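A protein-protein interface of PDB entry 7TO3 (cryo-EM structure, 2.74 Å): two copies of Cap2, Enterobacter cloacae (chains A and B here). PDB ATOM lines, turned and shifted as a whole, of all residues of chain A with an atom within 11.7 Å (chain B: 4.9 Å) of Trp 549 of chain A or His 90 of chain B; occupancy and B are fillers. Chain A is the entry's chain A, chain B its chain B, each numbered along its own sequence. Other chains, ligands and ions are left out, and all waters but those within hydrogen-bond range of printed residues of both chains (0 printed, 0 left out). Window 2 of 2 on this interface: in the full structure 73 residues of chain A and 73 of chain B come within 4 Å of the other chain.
Of the 15 printed residues of chain A, 3 touch a printed residue of chain B.
Hydrophobic or aromatic side chains of chain A that line the printed part of chain B: Trp 549 and His 550.
Of the 15 printed residues of chain B, 4 touch a printed residue of chain A.
Hydrophobic or aromatic side chains of chain B within 4 Å of the printed part of chain A: His 90 and Ala 158.
Among the printed residues, 6 pairs touch across the chains.
Among the printed residues, no Asp or Glu carboxylate lies within 4 Å of a Lys or Arg side-chain nitrogen of the other chain.
N of Glu 544 of chain A lies close to O of His 550 of chain A (3.5 Å).
O of His 90 of chain B lies within hydrogen-bond range of N of Ala 109 of chain B.
The backbone carbonyl oxygen (O) of His 90 of chain B is in hydrogen-bond range of the indole nitrogen (NE1) of Trp 143 of chain B.
Among the printed residues, pairs that only touch across the chains: Ala 548 of chain A with Ala 158 of chain B, Trp 549 of chain A with His 90 of chain B, Trp 549 of chain A with Asn 112 of chain B, Trp 549 of chain A with Ala 158 of chain B, Trp 549 of chain A with Glu 160 of chain B and His 550 of chain A with Asn 112 of chain B.
Printed residues of chain B within 4 Å of Trp 549 of chain A: His 90 (3.6 Å), Asn 112 (3.9 Å), Ala 158 (3.7 Å) and Glu 160 (3.4 Å).
No residue of chain A comes within 4 Å of Gln 89 of chain B.
No residue of chain A comes within 4 Å of Gln 91 of chain B.
No residue of chain A comes within 4 Å of Pro 108 of chain B.
Ala 109 of chain B touches none of the printed residues of chain A.
Of chain A, only Trp 549 and His 550 come within 4 Å of Asn 112 of chain B.
No residue of chain A comes within 4 Å of Pro 114 of chain B.
Leu 152 of chain B touches none of the printed residues of chain A.
Ala 158 of chain B touches two residues of chain A.
Glu 160 of chain B touches just one residue of chain A: Trp 549.
Printed residues of chain B within 4 Å of His 550 of chain A: Asn 112 (3.9 Å).
Of the printed residues of chain B, Ala 548 of chain A touches Ala 158 (3.9 Å).
The nearest residue of chain A that does not touch His 90 of chain B is His 550 of chain A (7.8 Å).
No position is printed for both chains.
Of the 6 pairs that touch across the chains among the printed residues, none has its exchanged pair printed and touching as well.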
ATOM      1  N   MET A 538     -21.947   5.904  -5.427  1.00  0.00           N
ATOM      2  CA  MET A 538     -22.236   5.509  -4.055  1.00  0.00           C
ATOM      3  C   MET A 538     -23.475   4.632  -3.928  1.00  0.00           C
ATOM      4  O   MET A 538     -23.704   4.071  -2.850  1.00  0.00           O
ATOM      5  CB  MET A 538     -22.395   6.751  -3.174  1.00  0.00           C
ATOM      6  CG  MET A 538     -21.143   7.606  -3.078  1.00  0.00           C
ATOM      7  SD  MET A 538     -19.697   6.660  -2.561  1.00  0.00           S
ATOM      8  CE  MET A 538     -20.143   6.254  -0.875  1.00  0.00           C
ATOM      9  N   GLU A 540     -24.103   1.723  -5.421  1.00  0.00           N
ATOM     10  CA  GLU A 540     -23.693   0.330  -5.283  1.00  0.00           C
ATOM     11  C   GLU A 540     -22.897   0.084  -4.007  1.00  0.00           C
ATOM     12  O   GLU A 540     -22.734  -1.075  -3.610  1.00  0.00           O
ATOM     13  CB  GLU A 540     -22.869  -0.104  -6.496  1.00  0.00           C
ATOM     14  CG  GLU A 540     -23.652  -0.167  -7.799  1.00  0.00           C
ATOM     15  CD  GLU A 540     -23.747   1.180  -8.488  1.00  0.00           C
ATOM     16  OE1 GLU A 540     -23.171   2.157  -7.965  1.00  0.00           O
ATOM     17  OE2 GLU A 540     -24.395   1.261  -9.552  1.00  0.00           O
ATOM     18  N   ALA A 541     -22.403   1.138  -3.362  1.00  0.00           N
ATOM     19  CA  ALA A 541     -21.597   0.986  -2.156  1.00  0.00           C
ATOM     20  C   ALA A 541     -22.501   0.644  -0.978  1.00  0.00           C
ATOM     21  O   ALA A 541     -23.257   1.493  -0.496  1.00  0.00           O
ATOM     22  CB  ALA A 541     -20.807   2.263  -1.886  1.00  0.00           C
ATOM     23  N   ARG A 542     -22.424  -0.598  -0.513  1.00  0.00           N
ATOM     24  CA  ARG A 542     -23.204  -1.030   0.635  1.00  0.00           C
ATOM     25  C   ARG A 542     -22.462  -0.725   1.931  1.00  0.00           C
ATOM     26  O   ARG A 542     -21.229  -0.727   1.981  1.00  0.00           O
ATOM     27  CB  ARG A 542     -23.508  -2.526   0.550  1.00  0.00           C
ATOM     28  CG  ARG A 542     -24.261  -2.942  -0.703  1.00  0.00           C
ATOM     29  CD  ARG A 542     -24.167  -4.442  -0.934  1.00  0.00           C
ATOM     30  NE  ARG A 542     -24.844  -5.204   0.108  1.00  0.00           N
ATOM     31  CZ  ARG A 542     -24.878  -6.529   0.165  1.00  0.00           C
ATOM     32  NH1 ARG A 542     -24.279  -7.275  -0.749  1.00  0.00           N
ATOM     33  NH2 ARG A 542     -25.526  -7.119   1.165  1.00  0.00           N
ATOM     34  N   ILE A 543     -23.232  -0.454   2.985  1.00  0.00           N
ATOM     35  CA  ILE A 543     -22.639  -0.229   4.296  1.00  0.00           C
ATOM     36  C   ILE A 543     -22.094  -1.547   4.836  1.00  0.00           C
ATOM     37  O   ILE A 543     -22.641  -2.628   4.575  1.00  0.00           O
ATOM     38  CB  ILE A 543     -23.670   0.393   5.256  1.00  0.00           C
ATOM     39  CG1 ILE A 543     -24.349   1.593   4.595  1.00  0.00           C
ATOM     40  CG2 ILE A 543     -23.009   0.827   6.556  1.00  0.00           C
ATOM     41  CD1 ILE A 543     -23.411   2.746   4.308  1.00  0.00           C
ATOM     42  N   GLU A 544     -20.994  -1.460   5.590  1.00  0.00           N
ATOM     43  CA  GLU A 544     -20.330  -2.664   6.081  1.00  0.00           C
ATOM     44  C   GLU A 544     -21.232  -3.481   6.999  1.00  0.00           C
ATOM     45  O   GLU A 544     -21.052  -4.698   7.121  1.00  0.00           O
ATOM     46  CB  GLU A 544     -19.036  -2.292   6.806  1.00  0.00           C
ATOM     47  CG  GLU A 544     -19.182  -1.132   7.774  1.00  0.00           C
ATOM     48  CD  GLU A 544     -17.863  -0.443   8.066  1.00  0.00           C
ATOM     49  OE1 GLU A 544     -16.821  -0.915   7.565  1.00  0.00           O
ATOM     50  OE2 GLU A 544     -17.869   0.567   8.800  1.00  0.00           O
ATOM     51  N   GLY A 545     -22.197  -2.842   7.648  1.00  0.00           N
ATOM     52  CA  GLY A 545     -23.105  -3.562   8.517  1.00  0.00           C
ATOM     53  C   GLY A 545     -24.008  -2.605   9.266  1.00  0.00           C
ATOM     54  O   GLY A 545     -23.987  -1.392   9.040  1.00  0.00           O
ATOM     55  N   ILE A 546     -24.803  -3.178  10.163  1.00  0.00           N
ATOM     56  CA  ILE A 546     -25.714  -2.395  10.989  1.00  0.00           C
ATOM     57  C   ILE A 546     -24.921  -1.702  12.090  1.00  0.00           C
ATOM     58  O   ILE A 546     -23.931  -2.240  12.601  1.00  0.00           O
ATOM     59  CB  ILE A 546     -26.830  -3.291  11.563  1.00  0.00           C
ATOM     60  CG1 ILE A 546     -27.952  -2.439  12.160  1.00  0.00           C
ATOM     61  CG2 ILE A 546     -26.276  -4.271  12.590  1.00  0.00           C
ATOM     62  CD1 ILE A 546     -29.174  -3.236  12.565  1.00  0.00           C
ATOM     63  N   GLY A 547     -25.342  -0.490  12.441  1.00  0.00           N
ATOM     64  CA  GLY A 547     -24.625   0.276  13.441  1.00  0.00           C
ATOM     65  C   GLY A 547     -23.303   0.837  12.975  1.00  0.00           C
ATOM     66  O   GLY A 547     -22.443   1.143  13.806  1.00  0.00           O
ATOM     67  N   ALA A 548     -23.111   0.980  11.665  1.00  0.00           N
ATOM     68  CA  ALA A 548     -21.871   1.489  11.098  1.00  0.00           C
ATOM     69  C   ALA A 548     -22.184   2.613  10.120  1.00  0.00           C
ATOM     70  O   ALA A 548     -23.341   2.864   9.771  1.00  0.00           O
ATOM     71  CB  ALA A 548     -21.077   0.376  10.404  1.00  0.00           C
ATOM     72  N   TRP A 549     -21.130   3.297   9.677  1.00  0.00           N
ATOM     73  CA  TRP A 549     -21.285   4.461   8.812  1.00  0.00           C
ATOM     74  C   TRP A 549     -20.532   4.327   7.493  1.00  0.00           C
ATOM     75  O   TRP A 549     -21.060   4.708   6.444  1.00  0.00           O
ATOM     76  CB  TRP A 549     -20.815   5.718   9.552  1.00  0.00           C
ATOM     77  CG  TRP A 549     -20.849   6.964   8.724  1.00  0.00           C
ATOM     78  CD1 TRP A 549     -19.795   7.561   8.098  1.00  0.00           C
ATOM     79  CD2 TRP A 549     -21.995   7.778   8.444  1.00  0.00           C
ATOM     80  NE1 TRP A 549     -20.212   8.691   7.439  1.00  0.00           N
ATOM     81  CE2 TRP A 549     -21.560   8.847   7.636  1.00  0.00           C
ATOM     82  CE3 TRP A 549     -23.346   7.704   8.796  1.00  0.00           C
ATOM     83  CZ2 TRP A 549     -22.427   9.835   7.174  1.00  0.00           C
ATOM     84  CZ3 TRP A 549     -24.205   8.685   8.335  1.00  0.00           C
ATOM     85  CH2 TRP A 549     -23.742   9.737   7.534  1.00  0.00           C
ATOM     86  N   HIS A 550     -19.313   3.798   7.525  1.00  0.00           N
ATOM     87  CA  HIS A 550     -18.490   3.760   6.324  1.00  0.00           C
ATOM     88  C   HIS A 550     -18.953   2.647   5.386  1.00  0.00           C
ATOM     89  O   HIS A 550     -19.296   1.551   5.841  1.00  0.00           O
ATOM     90  CB  HIS A 550     -17.021   3.556   6.690  1.00  0.00           C
ATOM     91  CG  HIS A 550     -16.497   4.562   7.667  1.00  0.00           C
ATOM     92  ND1 HIS A 550     -16.134   5.839   7.298  1.00  0.00           N
ATOM     93  CD2 HIS A 550     -16.276   4.477   9.000  1.00  0.00           C
ATOM     94  CE1 HIS A 550     -15.711   6.499   8.361  1.00  0.00           C
ATOM     95  NE2 HIS A 550     -15.788   5.695   9.408  1.00  0.00           N
ATOM     96  N   PRO A 551     -18.975   2.895   4.080  1.00  0.00           N
ATOM     97  CA  PRO A 551     -19.313   1.837   3.124  1.00  0.00           C
ATOM     98  C   PRO A 551     -18.083   1.027   2.733  1.00  0.00           C
ATOM     99  O   PRO A 551     -16.964   1.275   3.184  1.00  0.00           O
ATOM    100  CB  PRO A 551     -19.865   2.619   1.930  1.00  0.00           C
ATOM    101  CG  PRO A 551     -19.101   3.904   1.966  1.00  0.00           C
ATOM    102  CD  PRO A 551     -18.831   4.207   3.425  1.00  0.00           C
ATOM    103  N   VAL A 552     -18.316   0.038   1.871  1.00  0.00           N
ATOM    104  CA  VAL A 552     -17.266  -0.839   1.371  1.00  0.00           C
ATOM    105  C   VAL A 552     -17.364  -0.898  -0.148  1.00  0.00           C
ATOM    106  O   VAL A 552     -18.411  -0.620  -0.739  1.00  0.00           O
ATOM    107  CB  VAL A 552     -17.353  -2.254   1.977  1.00  0.00           C
ATOM    108  CG1 VAL A 552     -17.016  -2.221   3.460  1.00  0.00           C
ATOM    109  CG2 VAL A 552     -18.736  -2.844   1.750  1.00  0.00           C
ATOM    110  N   PHE A 553     -16.252  -1.266  -0.783  1.00  0.00           N
ATOM    111  CA  PHE A 553     -16.240  -1.346  -2.241  1.00  0.00           C
ATOM    112  C   PHE A 553     -16.677  -2.736  -2.693  1.00  0.00           C
ATOM    113  O   PHE A 553     -16.242  -3.736  -2.113  1.00  0.00           O
ATOM    114  CB  PHE A 553     -14.858  -0.995  -2.802  1.00  0.00           C
ATOM    115  CG  PHE A 553     -13.800  -2.035  -2.551  1.00  0.00           C
ATOM    116  CD1 PHE A 553     -13.070  -2.032  -1.373  1.00  0.00           C
ATOM    117  CD2 PHE A 553     -13.510  -2.995  -3.508  1.00  0.00           C
ATOM    118  CE1 PHE A 553     -12.087  -2.977  -1.146  1.00  0.00           C
ATOM    119  CE2 PHE A 553     -12.531  -3.945  -3.285  1.00  0.00           C
ATOM    120  CZ  PHE A 553     -11.818  -3.935  -2.103  1.00  0.00           C
ATOM    121  N   PHE B  88     -21.346  14.929  20.258  1.00  0.00           N
ATOM    122  CA  PHE B  88     -22.370  14.906  19.227  1.00  0.00           C
ATOM    123  C   PHE B  88     -22.074  13.786  18.231  1.00  0.00           C
ATOM    124  O   PHE B  88     -21.157  12.978  18.421  1.00  0.00           O
ATOM    125  CB  PHE B  88     -22.451  16.265  18.527  1.00  0.00           C
ATOM    126  CG  PHE B  88     -22.719  17.416  19.456  1.00  0.00           C
ATOM    127  CD1 PHE B  88     -21.678  18.056  20.108  1.00  0.00           C
ATOM    128  CD2 PHE B  88     -24.013  17.861  19.671  1.00  0.00           C
ATOM    129  CE1 PHE B  88     -21.922  19.115  20.961  1.00  0.00           C
ATOM    130  CE2 PHE B  88     -24.263  18.921  20.522  1.00  0.00           C
ATOM    131  CZ  PHE B  88     -23.216  19.549  21.168  1.00  0.00           C
ATOM    132  N   GLN B  89     -22.864  13.736  17.163  1.00  0.00           N
ATOM    133  CA  GLN B  89     -22.600  12.812  16.074  1.00  0.00           C
ATOM    134  C   GLN B  89     -21.392  13.281  15.266  1.00  0.00           C
ATOM    135  O   GLN B  89     -21.044  14.465  15.251  1.00  0.00           O
ATOM    136  CB  GLN B  89     -23.823  12.682  15.164  1.00  0.00           C
ATOM    137  CG  GLN B  89     -25.010  11.987  15.810  1.00  0.00           C
ATOM    138  CD  GLN B  89     -25.996  12.963  16.421  1.00  0.00           C
ATOM    139  OE1 GLN B  89     -25.754  14.170  16.453  1.00  0.00           O
ATOM    140  NE2 GLN B  89     -27.117  12.444  16.908  1.00  0.00           N
ATOM    141  N   HIS B  90     -20.755  12.327  14.585  1.00  0.00           N
ATOM    142  CA  HIS B  90     -19.567  12.589  13.771  1.00  0.00           C
ATOM    143  C   HIS B  90     -18.475  13.264  14.599  1.00  0.00           C
ATOM    144  O   HIS B  90     -17.885  14.270  14.200  1.00  0.00           O
ATOM    145  CB  HIS B  90     -19.919  13.427  12.540  1.00  0.00           C
ATOM    146  CG  HIS B  90     -21.043  12.866  11.728  1.00  0.00           C
ATOM    147  ND1 HIS B  90     -20.885  11.792  10.878  1.00  0.00           N
ATOM    148  CD2 HIS B  90     -22.345  13.229  11.635  1.00  0.00           C
ATOM    149  CE1 HIS B  90     -22.039  11.519  10.296  1.00  0.00           C
ATOM    150  NE2 HIS B  90     -22.942  12.376  10.738  1.00  0.00           N
ATOM    151  N   GLN B  91     -18.208  12.695  15.772  1.00  0.00           N
ATOM    152  CA  GLN B  91     -17.241  13.271  16.695  1.00  0.00           C
ATOM    153  C   GLN B  91     -16.772  12.193  17.661  1.00  0.00           C
ATOM    154  O   GLN B  91     -17.537  11.300  18.033  1.00  0.00           O
ATOM    155  CB  GLN B  91     -17.848  14.453  17.463  1.00  0.00           C
ATOM    156  CG  GLN B  91     -16.871  15.204  18.353  1.00  0.00           C
ATOM    157  CD  GLN B  91     -17.570  16.143  19.316  1.00  0.00           C
ATOM    158  OE1 GLN B  91     -18.791  16.098  19.467  1.00  0.00           O
ATOM    159  NE2 GLN B  91     -16.798  16.999  19.974  1.00  0.00           N
ATOM    160  N   ASN B  92     -15.505  12.287  18.058  1.00  0.00           N
ATOM    161  CA  ASN B  92     -14.962  11.391  19.064  1.00  0.00           C
ATOM    162  C   ASN B  92     -15.408  11.830  20.457  1.00  0.00           C
ATOM    163  O   ASN B  92     -15.937  12.927  20.655  1.00  0.00           O
ATOM    164  CB  ASN B  92     -13.437  11.347  18.977  1.00  0.00           C
ATOM    165  CG  ASN B  92     -12.944  10.718  17.688  1.00  0.00           C
ATOM    166  OD1 ASN B  92     -13.733  10.207  16.893  1.00  0.00           O
ATOM    167  ND2 ASN B  92     -11.634  10.752  17.476  1.00  0.00           N
ATOM    168  N   PRO B 108     -13.933  16.805  16.239  1.00  0.00           N
ATOM    169  CA  PRO B 108     -15.005  16.497  15.283  1.00  0.00           C
ATOM    170  C   PRO B 108     -14.453  15.785  14.057  1.00  0.00           C
ATOM    171  O   PRO B 108     -13.373  16.116  13.563  1.00  0.00           O
ATOM    172  CB  PRO B 108     -15.577  17.876  14.928  1.00  0.00           C
ATOM    173  CG  PRO B 108     -15.093  18.795  16.014  1.00  0.00           C
ATOM    174  CD  PRO B 108     -13.764  18.254  16.431  1.00  0.00           C
ATOM    175  N   ALA B 109     -15.208  14.806  13.564  1.00  0.00           N
ATOM    176  CA  ALA B 109     -14.832  14.064  12.361  1.00  0.00           C
ATOM    177  C   ALA B 109     -15.292  14.867  11.151  1.00  0.00           C
ATOM    178  O   ALA B 109     -16.368  14.642  10.597  1.00  0.00           O
ATOM    179  CB  ALA B 109     -15.437  12.667  12.375  1.00  0.00           C
ATOM    180  N   ASN B 112     -16.190  13.077   7.532  1.00  0.00           N
ATOM    181  CA  ASN B 112     -17.520  12.544   7.270  1.00  0.00           C
ATOM    182  C   ASN B 112     -18.439  13.651   6.767  1.00  0.00           C
ATOM    183  O   ASN B 112     -18.385  14.785   7.251  1.00  0.00           O
ATOM    184  CB  ASN B 112     -18.095  11.905   8.534  1.00  0.00           C
ATOM    185  CG  ASN B 112     -17.261  10.740   9.027  1.00  0.00           C
ATOM    186  OD1 ASN B 112     -16.314  10.314   8.365  1.00  0.00           O
ATOM    187  ND2 ASN B 112     -17.609  10.215  10.195  1.00  0.00           N
ATOM    188  N   THR B 113     -19.286  13.319   5.793  1.00  0.00           N
ATOM    189  CA  THR B 113     -20.157  14.302   5.156  1.00  0.00           C
ATOM    190  C   THR B 113     -21.613  14.011   5.496  1.00  0.00           C
ATOM    191  O   THR B 113     -22.225  13.116   4.893  1.00  0.00           O
ATOM    192  CB  THR B 113     -19.955  14.298   3.638  1.00  0.00           C
ATOM    193  OG1 THR B 113     -20.208  12.984   3.125  1.00  0.00           O
ATOM    194  CG2 THR B 113     -18.532  14.703   3.288  1.00  0.00           C
ATOM    195  N   PRO B 114     -22.213  14.729   6.443  1.00  0.00           N
ATOM    196  CA  PRO B 114     -23.643  14.552   6.713  1.00  0.00           C
ATOM    197  C   PRO B 114     -24.493  15.156   5.605  1.00  0.00           C
ATOM    198  O   PRO B 114     -24.001  15.805   4.679  1.00  0.00           O
ATOM    199  CB  PRO B 114     -23.855  15.285   8.044  1.00  0.00           C
ATOM    200  CG  PRO B 114     -22.473  15.492   8.609  1.00  0.00           C
ATOM    201  CD  PRO B 114     -21.574  15.620   7.423  1.00  0.00           C
ATOM    202  N   TRP B 143     -19.917  22.178  10.726  1.00  0.00           N
ATOM    203  CA  TRP B 143     -20.230  21.168  11.731  1.00  0.00           C
ATOM    204  C   TRP B 143     -20.774  21.798  13.004  1.00  0.00           C
ATOM    205  O   TRP B 143     -21.717  21.273  13.605  1.00  0.00           O
ATOM    206  CB  TRP B 143     -18.986  20.335  12.041  1.00  0.00           C
ATOM    207  CG  TRP B 143     -19.244  19.206  12.995  1.00  0.00           C
ATOM    208  CD1 TRP B 143     -19.585  17.925  12.673  1.00  0.00           C
ATOM    209  CD2 TRP B 143     -19.180  19.256  14.426  1.00  0.00           C
ATOM    210  NE1 TRP B 143     -19.739  17.175  13.814  1.00  0.00           N
ATOM    211  CE2 TRP B 143     -19.495  17.969  14.903  1.00  0.00           C
ATOM    212  CE3 TRP B 143     -18.887  20.266  15.349  1.00  0.00           C
ATOM    213  CZ2 TRP B 143     -19.525  17.664  16.263  1.00  0.00           C
ATOM    214  CZ3 TRP B 143     -18.918  19.960  16.699  1.00  0.00           C
ATOM    215  CH2 TRP B 143     -19.235  18.671  17.142  1.00  0.00           C
ATOM    216  N   LEU B 152     -27.370  17.242  12.830  1.00  0.00           N
ATOM    217  CA  LEU B 152     -26.267  16.437  12.313  1.00  0.00           C
ATOM    218  C   LEU B 152     -26.777  15.144  11.691  1.00  0.00           C
ATOM    219  O   LEU B 152     -26.286  14.714  10.642  1.00  0.00           O
ATOM    220  CB  LEU B 152     -25.264  16.141  13.427  1.00  0.00           C
ATOM    221  CG  LEU B 152     -24.238  17.236  13.721  1.00  0.00           C
ATOM    222  CD1 LEU B 152     -23.454  16.911  14.983  1.00  0.00           C
ATOM    223  CD2 LEU B 152     -23.303  17.424  12.538  1.00  0.00           C
ATOM    224  N   ASP B 157     -30.006   9.301   6.664  1.00  0.00           N
ATOM    225  CA  ASP B 157     -28.683   8.963   7.161  1.00  0.00           C
ATOM    226  C   ASP B 157     -28.703   7.612   7.872  1.00  0.00           C
ATOM    227  O   ASP B 157     -29.743   7.137   8.337  1.00  0.00           O
ATOM    228  CB  ASP B 157     -28.171  10.045   8.113  1.00  0.00           C
ATOM    229  CG  ASP B 157     -27.741  11.305   7.387  1.00  0.00           C
ATOM    230  OD1 ASP B 157     -27.464  11.227   6.172  1.00  0.00           O
ATOM    231  OD2 ASP B 157     -27.679  12.372   8.033  1.00  0.00           O
ATOM    232  N   ALA B 158     -27.529   6.993   7.950  1.00  0.00           N
ATOM    233  CA  ALA B 158     -27.383   5.728   8.653  1.00  0.00           C
ATOM    234  C   ALA B 158     -27.267   5.967  10.153  1.00  0.00           C
ATOM    235  O   ALA B 158     -26.704   6.972  10.596  1.00  0.00           O
ATOM    236  CB  ALA B 158     -26.155   4.971   8.147  1.00  0.00           C
ATOM    237  N   GLU B 160     -25.434   5.455  12.993  1.00  0.00           N
ATOM    238  CA  GLU B 160     -24.143   5.029  13.513  1.00  0.00           C
ATOM    239  C   GLU B 160     -24.189   4.937  15.032  1.00  0.00           C
ATOM    240  O   GLU B 160     -24.763   5.797  15.706  1.00  0.00           O
ATOM    241  CB  GLU B 160     -23.043   5.997  13.078  1.00  0.00           C
ATOM    242  CG  GLU B 160     -21.636   5.478  13.328  1.00  0.00           C
ATOM    243  CD  GLU B 160     -20.563   6.445  12.868  1.00  0.00           C
ATOM    244  OE1 GLU B 160     -20.913   7.572  12.459  1.00  0.00           O
ATOM    245  OE2 GLU B 160     -19.371   6.078  12.915  1.00  0.00           O
